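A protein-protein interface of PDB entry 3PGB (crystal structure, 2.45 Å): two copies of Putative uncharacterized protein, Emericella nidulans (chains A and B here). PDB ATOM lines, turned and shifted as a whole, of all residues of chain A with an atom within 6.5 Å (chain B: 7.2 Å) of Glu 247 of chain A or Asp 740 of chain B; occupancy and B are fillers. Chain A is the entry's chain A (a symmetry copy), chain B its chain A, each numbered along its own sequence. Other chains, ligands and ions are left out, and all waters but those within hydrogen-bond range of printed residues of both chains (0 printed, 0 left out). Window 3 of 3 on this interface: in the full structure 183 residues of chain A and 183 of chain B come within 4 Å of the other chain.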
ATOM      1  N   ALA A 244       9.985 -39.652  27.073  1.00  0.00           N
ATOM      2  CA  ALA A 244      10.118 -39.055  25.747  1.00  0.00           C
ATOM      3  C   ALA A 244      11.575 -38.745  25.486  1.00  0.00           C
ATOM      4  O   ALA A 244      12.366 -38.621  26.423  1.00  0.00           O
ATOM      5  CB  ALA A 244       9.290 -37.779  25.646  1.00  0.00           C
ATOM      6  N   ASP A 245      11.925 -38.612  24.210  1.00  0.00           N
ATOM      7  CA  ASP A 245      13.275 -38.207  23.818  1.00  0.00           C
ATOM      8  C   ASP A 245      13.542 -36.784  24.306  1.00  0.00           C
ATOM      9  O   ASP A 245      12.608 -36.032  24.604  1.00  0.00           O
ATOM     10  CB  ASP A 245      13.450 -38.284  22.297  1.00  0.00           C
ATOM     11  CG  ASP A 245      13.233 -39.696  21.740  1.00  0.00           C
ATOM     12  OD1 ASP A 245      13.470 -40.682  22.473  1.00  0.00           O
ATOM     13  OD2 ASP A 245      12.825 -39.810  20.559  1.00  0.00           O
ATOM     14  N   ASP A 246      14.817 -36.420  24.390  1.00  0.00           N
ATOM     15  CA  ASP A 246      15.209 -35.100  24.891  1.00  0.00           C
ATOM     16  C   ASP A 246      14.594 -33.988  24.043  1.00  0.00           C
ATOM     17  O   ASP A 246      14.668 -34.023  22.816  1.00  0.00           O
ATOM     18  CB  ASP A 246      16.737 -34.960  24.892  1.00  0.00           C
ATOM     19  CG  ASP A 246      17.425 -35.959  25.823  1.00  0.00           C
ATOM     20  OD1 ASP A 246      16.794 -36.394  26.816  1.00  0.00           O
ATOM     21  OD2 ASP A 246      18.603 -36.301  25.554  1.00  0.00           O
ATOM     22  N   GLU A 247      13.986 -33.007  24.703  1.00  0.00           N
ATOM     23  CA  GLU A 247      13.361 -31.864  24.020  1.00  0.00           C
ATOM     24  C   GLU A 247      12.103 -32.233  23.205  1.00  0.00           C
ATOM     25  O   GLU A 247      11.791 -31.597  22.192  1.00  0.00           O
ATOM     26  CB  GLU A 247      14.392 -31.071  23.170  1.00  0.00           C
ATOM     27  CG  GLU A 247      15.410 -30.280  24.019  1.00  0.00           C
ATOM     28  CD  GLU A 247      15.998 -29.067  23.294  1.00  0.00           C
ATOM     29  OE1 GLU A 247      15.574 -27.917  23.595  1.00  0.00           O
ATOM     30  OE2 GLU A 247      16.882 -29.263  22.423  1.00  0.00           O
ATOM     31  N   PHE A 248      11.386 -33.257  23.666  1.00  0.00           N
ATOM     32  CA  PHE A 248      10.022 -33.544  23.207  1.00  0.00           C
ATOM     33  C   PHE A 248       9.106 -33.756  24.420  1.00  0.00           C
ATOM     34  O   PHE A 248       9.552 -34.244  25.454  1.00  0.00           O
ATOM     35  CB  PHE A 248      10.007 -34.763  22.285  1.00  0.00           C
ATOM     36  CG  PHE A 248      10.640 -34.511  20.940  1.00  0.00           C
ATOM     37  CD1 PHE A 248       9.989 -33.729  19.988  1.00  0.00           C
ATOM     38  CD2 PHE A 248      11.889 -35.050  20.625  1.00  0.00           C
ATOM     39  CE1 PHE A 248      10.561 -33.491  18.745  1.00  0.00           C
ATOM     40  CE2 PHE A 248      12.475 -34.815  19.380  1.00  0.00           C
ATOM     41  CZ  PHE A 248      11.807 -34.033  18.439  1.00  0.00           C
ATOM     42  N   ASP A 249       7.836 -33.375  24.301  1.00  0.00           N
ATOM     43  CA  ASP A 249       6.904 -33.441  25.434  1.00  0.00           C
ATOM     44  C   ASP A 249       5.819 -34.506  25.210  1.00  0.00           C
ATOM     45  O   ASP A 249       4.623 -34.250  25.386  1.00  0.00           O
ATOM     46  CB  ASP A 249       6.274 -32.059  25.674  1.00  0.00           C
ATOM     47  CG  ASP A 249       5.730 -31.894  27.085  1.00  0.00           C
ATOM     48  OD1 ASP A 249       6.377 -32.358  28.043  1.00  0.00           O
ATOM     49  OD2 ASP A 249       4.655 -31.286  27.234  1.00  0.00           O
ATOM     50  N   TYR A 773      11.338 -14.018  21.605  1.00  0.00           N
ATOM     51  CA  TYR A 773      10.621 -14.770  22.630  1.00  0.00           C
ATOM     52  C   TYR A 773      11.549 -14.927  23.830  1.00  0.00           C
ATOM     53  O   TYR A 773      12.674 -15.417  23.686  1.00  0.00           O
ATOM     54  CB  TYR A 773      10.191 -16.148  22.101  1.00  0.00           C
ATOM     55  CG  TYR A 773       9.142 -16.845  22.948  1.00  0.00           C
ATOM     56  CD1 TYR A 773       9.503 -17.694  23.990  1.00  0.00           C
ATOM     57  CD2 TYR A 773       7.783 -16.663  22.692  1.00  0.00           C
ATOM     58  CE1 TYR A 773       8.538 -18.335  24.759  1.00  0.00           C
ATOM     59  CE2 TYR A 773       6.816 -17.300  23.456  1.00  0.00           C
ATOM     60  CZ  TYR A 773       7.198 -18.130  24.485  1.00  0.00           C
ATOM     61  OH  TYR A 773       6.232 -18.752  25.240  1.00  0.00           O
ATOM     62  N   THR B 461       5.863 -25.812  26.317  1.00  0.00           N
ATOM     63  CA  THR B 461       6.536 -26.348  27.504  1.00  0.00           C
ATOM     64  C   THR B 461       7.386 -25.235  28.112  1.00  0.00           C
ATOM     65  O   THR B 461       7.434 -24.124  27.580  1.00  0.00           O
ATOM     66  CB  THR B 461       7.445 -27.563  27.184  1.00  0.00           C
ATOM     67  OG1 THR B 461       8.618 -27.128  26.478  1.00  0.00           O
ATOM     68  CG2 THR B 461       6.711 -28.601  26.359  1.00  0.00           C
ATOM     69  N   GLU B 463      10.442 -25.120  27.934  1.00  0.00           N
ATOM     70  CA  GLU B 463      11.658 -25.073  27.108  1.00  0.00           C
ATOM     71  C   GLU B 463      11.418 -24.753  25.626  1.00  0.00           C
ATOM     72  O   GLU B 463      12.325 -24.268  24.951  1.00  0.00           O
ATOM     73  CB  GLU B 463      12.387 -26.407  27.217  1.00  0.00           C
ATOM     74  CG  GLU B 463      12.729 -26.802  28.648  1.00  0.00           C
ATOM     75  CD  GLU B 463      13.498 -28.113  28.734  1.00  0.00           C
ATOM     76  OE1 GLU B 463      13.575 -28.844  27.714  1.00  0.00           O
ATOM     77  OE2 GLU B 463      14.025 -28.411  29.835  1.00  0.00           O
ATOM     78  N   PHE B 464      10.217 -25.030  25.113  1.00  0.00           N
ATOM     79  CA  PHE B 464       9.889 -24.697  23.727  1.00  0.00           C
ATOM     80  C   PHE B 464       8.399 -24.535  23.484  1.00  0.00           C
ATOM     81  O   PHE B 464       7.568 -25.006  24.257  1.00  0.00           O
ATOM     82  CB  PHE B 464      10.450 -25.752  22.769  1.00  0.00           C
ATOM     83  CG  PHE B 464       9.809 -27.107  22.908  1.00  0.00           C
ATOM     84  CD1 PHE B 464       8.866 -27.544  21.982  1.00  0.00           C
ATOM     85  CD2 PHE B 464      10.151 -27.947  23.963  1.00  0.00           C
ATOM     86  CE1 PHE B 464       8.270 -28.794  22.106  1.00  0.00           C
ATOM     87  CE2 PHE B 464       9.563 -29.196  24.097  1.00  0.00           C
ATOM     88  CZ  PHE B 464       8.622 -29.621  23.163  1.00  0.00           C
ATOM     89  N   VAL B 465       8.071 -23.862  22.390  1.00  0.00           N
ATOM     90  CA  VAL B 465       6.686 -23.712  21.965  1.00  0.00           C
ATOM     91  C   VAL B 465       6.590 -24.018  20.480  1.00  0.00           C
ATOM     92  O   VAL B 465       7.502 -23.710  19.717  1.00  0.00           O
ATOM     93  CB  VAL B 465       6.173 -22.291  22.244  1.00  0.00           C
ATOM     94  CG1 VAL B 465       4.744 -22.117  21.731  1.00  0.00           C
ATOM     95  CG2 VAL B 465       6.250 -21.997  23.734  1.00  0.00           C
ATOM     96  N   ARG B 738       8.493 -23.749  15.448  1.00  0.00           N
ATOM     97  CA  ARG B 738       8.898 -24.214  16.775  1.00  0.00           C
ATOM     98  C   ARG B 738       9.994 -23.315  17.345  1.00  0.00           C
ATOM     99  O   ARG B 738      11.107 -23.285  16.819  1.00  0.00           O
ATOM    100  CB  ARG B 738       9.398 -25.656  16.721  1.00  0.00           C
ATOM    101  CG  ARG B 738       9.771 -26.246  18.090  1.00  0.00           C
ATOM    102  CD  ARG B 738      10.710 -27.433  17.937  1.00  0.00           C
ATOM    103  NE  ARG B 738      11.495 -27.681  19.148  1.00  0.00           N
ATOM    104  CZ  ARG B 738      11.364 -28.737  19.952  1.00  0.00           C
ATOM    105  NH1 ARG B 738      10.479 -29.694  19.703  1.00  0.00           N
ATOM    106  NH2 ARG B 738      12.141 -28.844  21.025  1.00  0.00           N
ATOM    107  N   VAL B 739       9.669 -22.591  18.417  1.00  0.00           N
ATOM    108  CA  VAL B 739      10.640 -21.757  19.120  1.00  0.00           C
ATOM    109  C   VAL B 739      11.158 -22.478  20.356  1.00  0.00           C
ATOM    110  O   VAL B 739      10.377 -22.825  21.240  1.00  0.00           O
ATOM    111  CB  VAL B 739      10.024 -20.428  19.580  1.00  0.00           C
ATOM    112  CG1 VAL B 739      11.120 -19.511  20.121  1.00  0.00           C
ATOM    113  CG2 VAL B 739       9.257 -19.759  18.442  1.00  0.00           C
ATOM    114  N   ASP B 740      12.468 -22.716  20.404  1.00  0.00           N
ATOM    115  CA  ASP B 740      13.130 -23.193  21.616  1.00  0.00           C
ATOM    116  C   ASP B 740      13.639 -21.970  22.370  1.00  0.00           C
ATOM    117  O   ASP B 740      14.079 -21.011  21.751  1.00  0.00           O
ATOM    118  CB  ASP B 740      14.285 -24.142  21.280  1.00  0.00           C
ATOM    119  CG  ASP B 740      13.806 -25.523  20.872  1.00  0.00           C
ATOM    120  OD1 ASP B 740      13.827 -26.444  21.713  1.00  0.00           O
ATOM    121  OD2 ASP B 740      13.392 -25.694  19.712  1.00  0.00           O
ATOM    122  N   TYR B 741      13.570 -21.987  23.698  1.00  0.00           N
ATOM    123  CA  TYR B 741      13.933 -20.796  24.475  1.00  0.00           C
ATOM    124  C   TYR B 741      14.507 -21.112  25.850  1.00  0.00           C
ATOM    125  O   TYR B 741      14.162 -22.123  26.460  1.00  0.00           O
ATOM    126  CB  TYR B 741      12.728 -19.863  24.617  1.00  0.00           C
ATOM    127  CG  TYR B 741      11.640 -20.385  25.524  1.00  0.00           C
ATOM    128  CD1 TYR B 741      11.594 -20.015  26.863  1.00  0.00           C
ATOM    129  CD2 TYR B 741      10.657 -21.246  25.048  1.00  0.00           C
ATOM    130  CE1 TYR B 741      10.605 -20.489  27.708  1.00  0.00           C
ATOM    131  CE2 TYR B 741       9.657 -21.725  25.887  1.00  0.00           C
ATOM    132  CZ  TYR B 741       9.641 -21.339  27.218  1.00  0.00           C
ATOM    133  OH  TYR B 741       8.661 -21.793  28.067  1.00  0.00           O
ATOM    134  N   SER B 742      15.391 -20.234  26.314  1.00  0.00           N
ATOM    135  CA  SER B 742      15.981 -20.325  27.654  1.00  0.00           C
ATOM    136  C   SER B 742      16.748 -19.047  27.990  1.00  0.00           C
ATOM    137  O   SER B 742      17.169 -18.300  27.093  1.00  0.00           O
ATOM    138  CB  SER B 742      16.913 -21.541  27.778  1.00  0.00           C
ATOM    139  OG  SER B 742      17.962 -21.489  26.829  1.00  0.00           O
ATOM    140  N   ALA B 745      15.871 -15.584  26.081  1.00  0.00           N
ATOM    141  CA  ALA B 745      15.921 -15.410  24.629  1.00  0.00           C
ATOM    142  C   ALA B 745      15.675 -16.727  23.907  1.00  0.00           C
ATOM    143  O   ALA B 745      15.808 -17.798  24.499  1.00  0.00           O
ATOM    144  CB  ALA B 745      17.270 -14.820  24.212  1.00  0.00           C
ATOM    145  N   ALA B 746      15.309 -16.631  22.631  1.00  0.00           N
ATOM    146  CA  ALA B 746      15.111 -17.808  21.783  1.00  0.00           C
ATOM    147  C   ALA B 746      16.455 -18.309  21.270  1.00  0.00           C
ATOM    148  O   ALA B 746      17.219 -17.538  20.676  1.00  0.00           O
ATOM    149  CB  ALA B 746      14.204 -17.470  20.616  1.00  0.00           C
ATOM    150  N   THR B 747      16.742 -19.592  21.499  1.00  0.00           N
ATOM    151  CA  THR B 747      17.976 -20.211  21.009  1.00  0.00           C
ATOM    152  C   THR B 747      17.834 -20.715  19.580  1.00  0.00           C
ATOM    153  O   THR B 747      18.809 -20.724  18.825  1.00  0.00           O
ATOM    154  CB  THR B 747      18.422 -21.388  21.893  1.00  0.00           C
ATOM    155  OG1 THR B 747      17.359 -22.338  22.010  1.00  0.00           O
ATOM    156  CG2 THR B 747      18.823 -20.896  23.279  1.00  0.00           C
ATOM    157  N   ALA B 748      16.629 -21.142  19.213  1.00  0.00           N
ATOM    158  CA  ALA B 748      16.363 -21.641  17.864  1.00  0.00           C
ATOM    159  C   ALA B 748      14.944 -21.294  17.413  1.00  0.00           C
ATOM    160  O   ALA B 748      14.021 -21.262  18.226  1.00  0.00           O
ATOM    161  CB  ALA B 748      16.586 -23.151  17.808  1.00  0.00           C
ATOM    162  N   VAL B 749      14.786 -21.019  16.122  1.00  0.00           N
ATOM    163  CA  VAL B 749      13.465 -20.836  15.513  1.00  0.00           C
ATOM    164  C   VAL B 749      13.381 -21.660  14.231  1.00  0.00           C
ATOM    165  O   VAL B 749      13.921 -21.268  13.199  1.00  0.00           O
ATOM    166  CB  VAL B 749      13.178 -19.366  15.163  1.00  0.00           C
ATOM    167  CG1 VAL B 749      11.783 -19.234  14.570  1.00  0.00           C
ATOM    168  CG2 VAL B 749      13.327 -18.485  16.385  1.00  0.00           C
ATOM    169  N   ARG B 750      12.716 -22.805  14.306  1.00  0.00           N
ATOM    170  CA  ARG B 750      12.542 -23.658  13.145  1.00  0.00           C
ATOM    171  C   ARG B 750      11.253 -23.251  12.427  1.00  0.00           C
ATOM    172  O   ARG B 750      10.189 -23.227  13.031  1.00  0.00           O
ATOM    173  CB  ARG B 750      12.511 -25.134  13.567  1.00  0.00           C
ATOM    174  CG  ARG B 750      12.942 -26.091  12.465  1.00  0.00           C
ATOM    175  CD  ARG B 750      13.036 -27.519  12.958  1.00  0.00           C
ATOM    176  NE  ARG B 750      13.172 -28.466  11.849  1.00  0.00           N
ATOM    177  CZ  ARG B 750      13.075 -29.791  11.967  1.00  0.00           C
ATOM    178  NH1 ARG B 750      12.836 -30.356  13.149  1.00  0.00           N
ATOM    179  NH2 ARG B 750      13.210 -30.564  10.893  1.00  0.00           N
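NH2 of Arg 738 of chain B is in hydrogen-bond range of O of Glu 247 of chain A (3.0 Å). OE1 of Glu 247 of chain A sits close to OD1 of Asp 740 of chain B, 3.0 Å away. The backbone carbonyl oxygen (O) of Tyr 773 of chain A is in hydrogen-bond range of the backbone NH (N) of Ala 746 of chain B, at 3.1 Å.
The backbone NH (N) of Arg 738 of chain B is in hydrogen-bond range of the backbone carbonyl oxygen (O) of Arg 750 of chain B (3.0 Å). O of Val 465 of chain B is in hydrogen-bond range of N of Val 739 of chain B (2.8 Å). The side-chain carboxylate (OD2) of Asp 740 of chain B is in salt-bridge range of the guanidinium group (NE) of Arg 738 of chain B (2.8 Å). N of Tyr 741 of chain B is in hydrogen-bond range of O of Glu 463 of chain B (2.9 Å). The backbone NH of Asp 740 of chain B is in hydrogen-bond range of the backbone carbonyl oxygen of Ala 748 of chain B. The backbone carbonyl oxygen (O) of Asp 740 of chain B sits at hydrogen-bond distance from the backbone NH (N) of Thr 747 of chain B, at 3.0 Å.
Among the printed residues, pairs that only touch across the chains: Tyr 773 of chain A with Ala 745 of chain B (3.3 Å), Asp 249 of chain A with Thr 461 of chain B (3.5 Å), Tyr 773 of chain A with Val 465 of chain B (3.6 Å), Tyr 773 of chain A with Tyr 741 of chain B (3.6 Å), Glu 247 of chain A with Phe 464 of chain B (3.8 Å) and Phe 248 of chain A with Arg 738 of chain B (3.9 Å).
Ala 244 of chain A touches none of the printed residues of chain B. Glu 247 of chain A touches just these residues of chain B: Phe 464 (3.8 Å), Arg 738 (3.0 Å) and Asp 740 (3.0 Å). Of the printed residues of chain B, Phe 248 of chain A touches Arg 738. Printed residues of chain B within 4 Å of Tyr 773 of chain A: Val 465, Tyr 741, Ala 745 and Ala 746. Of the printed residues of chain A, Thr 461 of chain B touches Asp 249 (3.5 Å). Of the printed residues of chain A, Phe 464 of chain B touches Glu 247. Printed residues of chain A within 4 Å of Arg 738 of chain B: Glu 247 (3.0 Å) and Phe 248 (3.9 Å). Asp 740 of chain B touches just one residue of chain A: Glu 247 (3.0 Å). The nearest residue of chain B that does not touch Glu 247 of chain A is Glu 463 of chain B (4.4 Å).
Of the 7 printed residues of chain A, 4 touch a printed residue of chain B. Printed residues of chain A that touch a printed residue of chain B: Glu 247, Phe 248, Asp 249 and Tyr 773. Hydrophobic or aromatic side chains of chain A that line the printed part of chain B: Phe 248 and Tyr 773. Along chain A the printed residues that touch a printed residue of chain B span positions 247 to 773. Of the 15 printed residues of chain B, 8 touch a printed residue of chain A. Hydrophobic or aromatic side chains of chain B that line the printed part of chain A: Phe 464, Val 465, Tyr 741 and Ala 746.
No position is printed for both chains. Of the 9 pairs that touch across the chains among the printed residues, none has its exchanged pair printed and touching as well.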
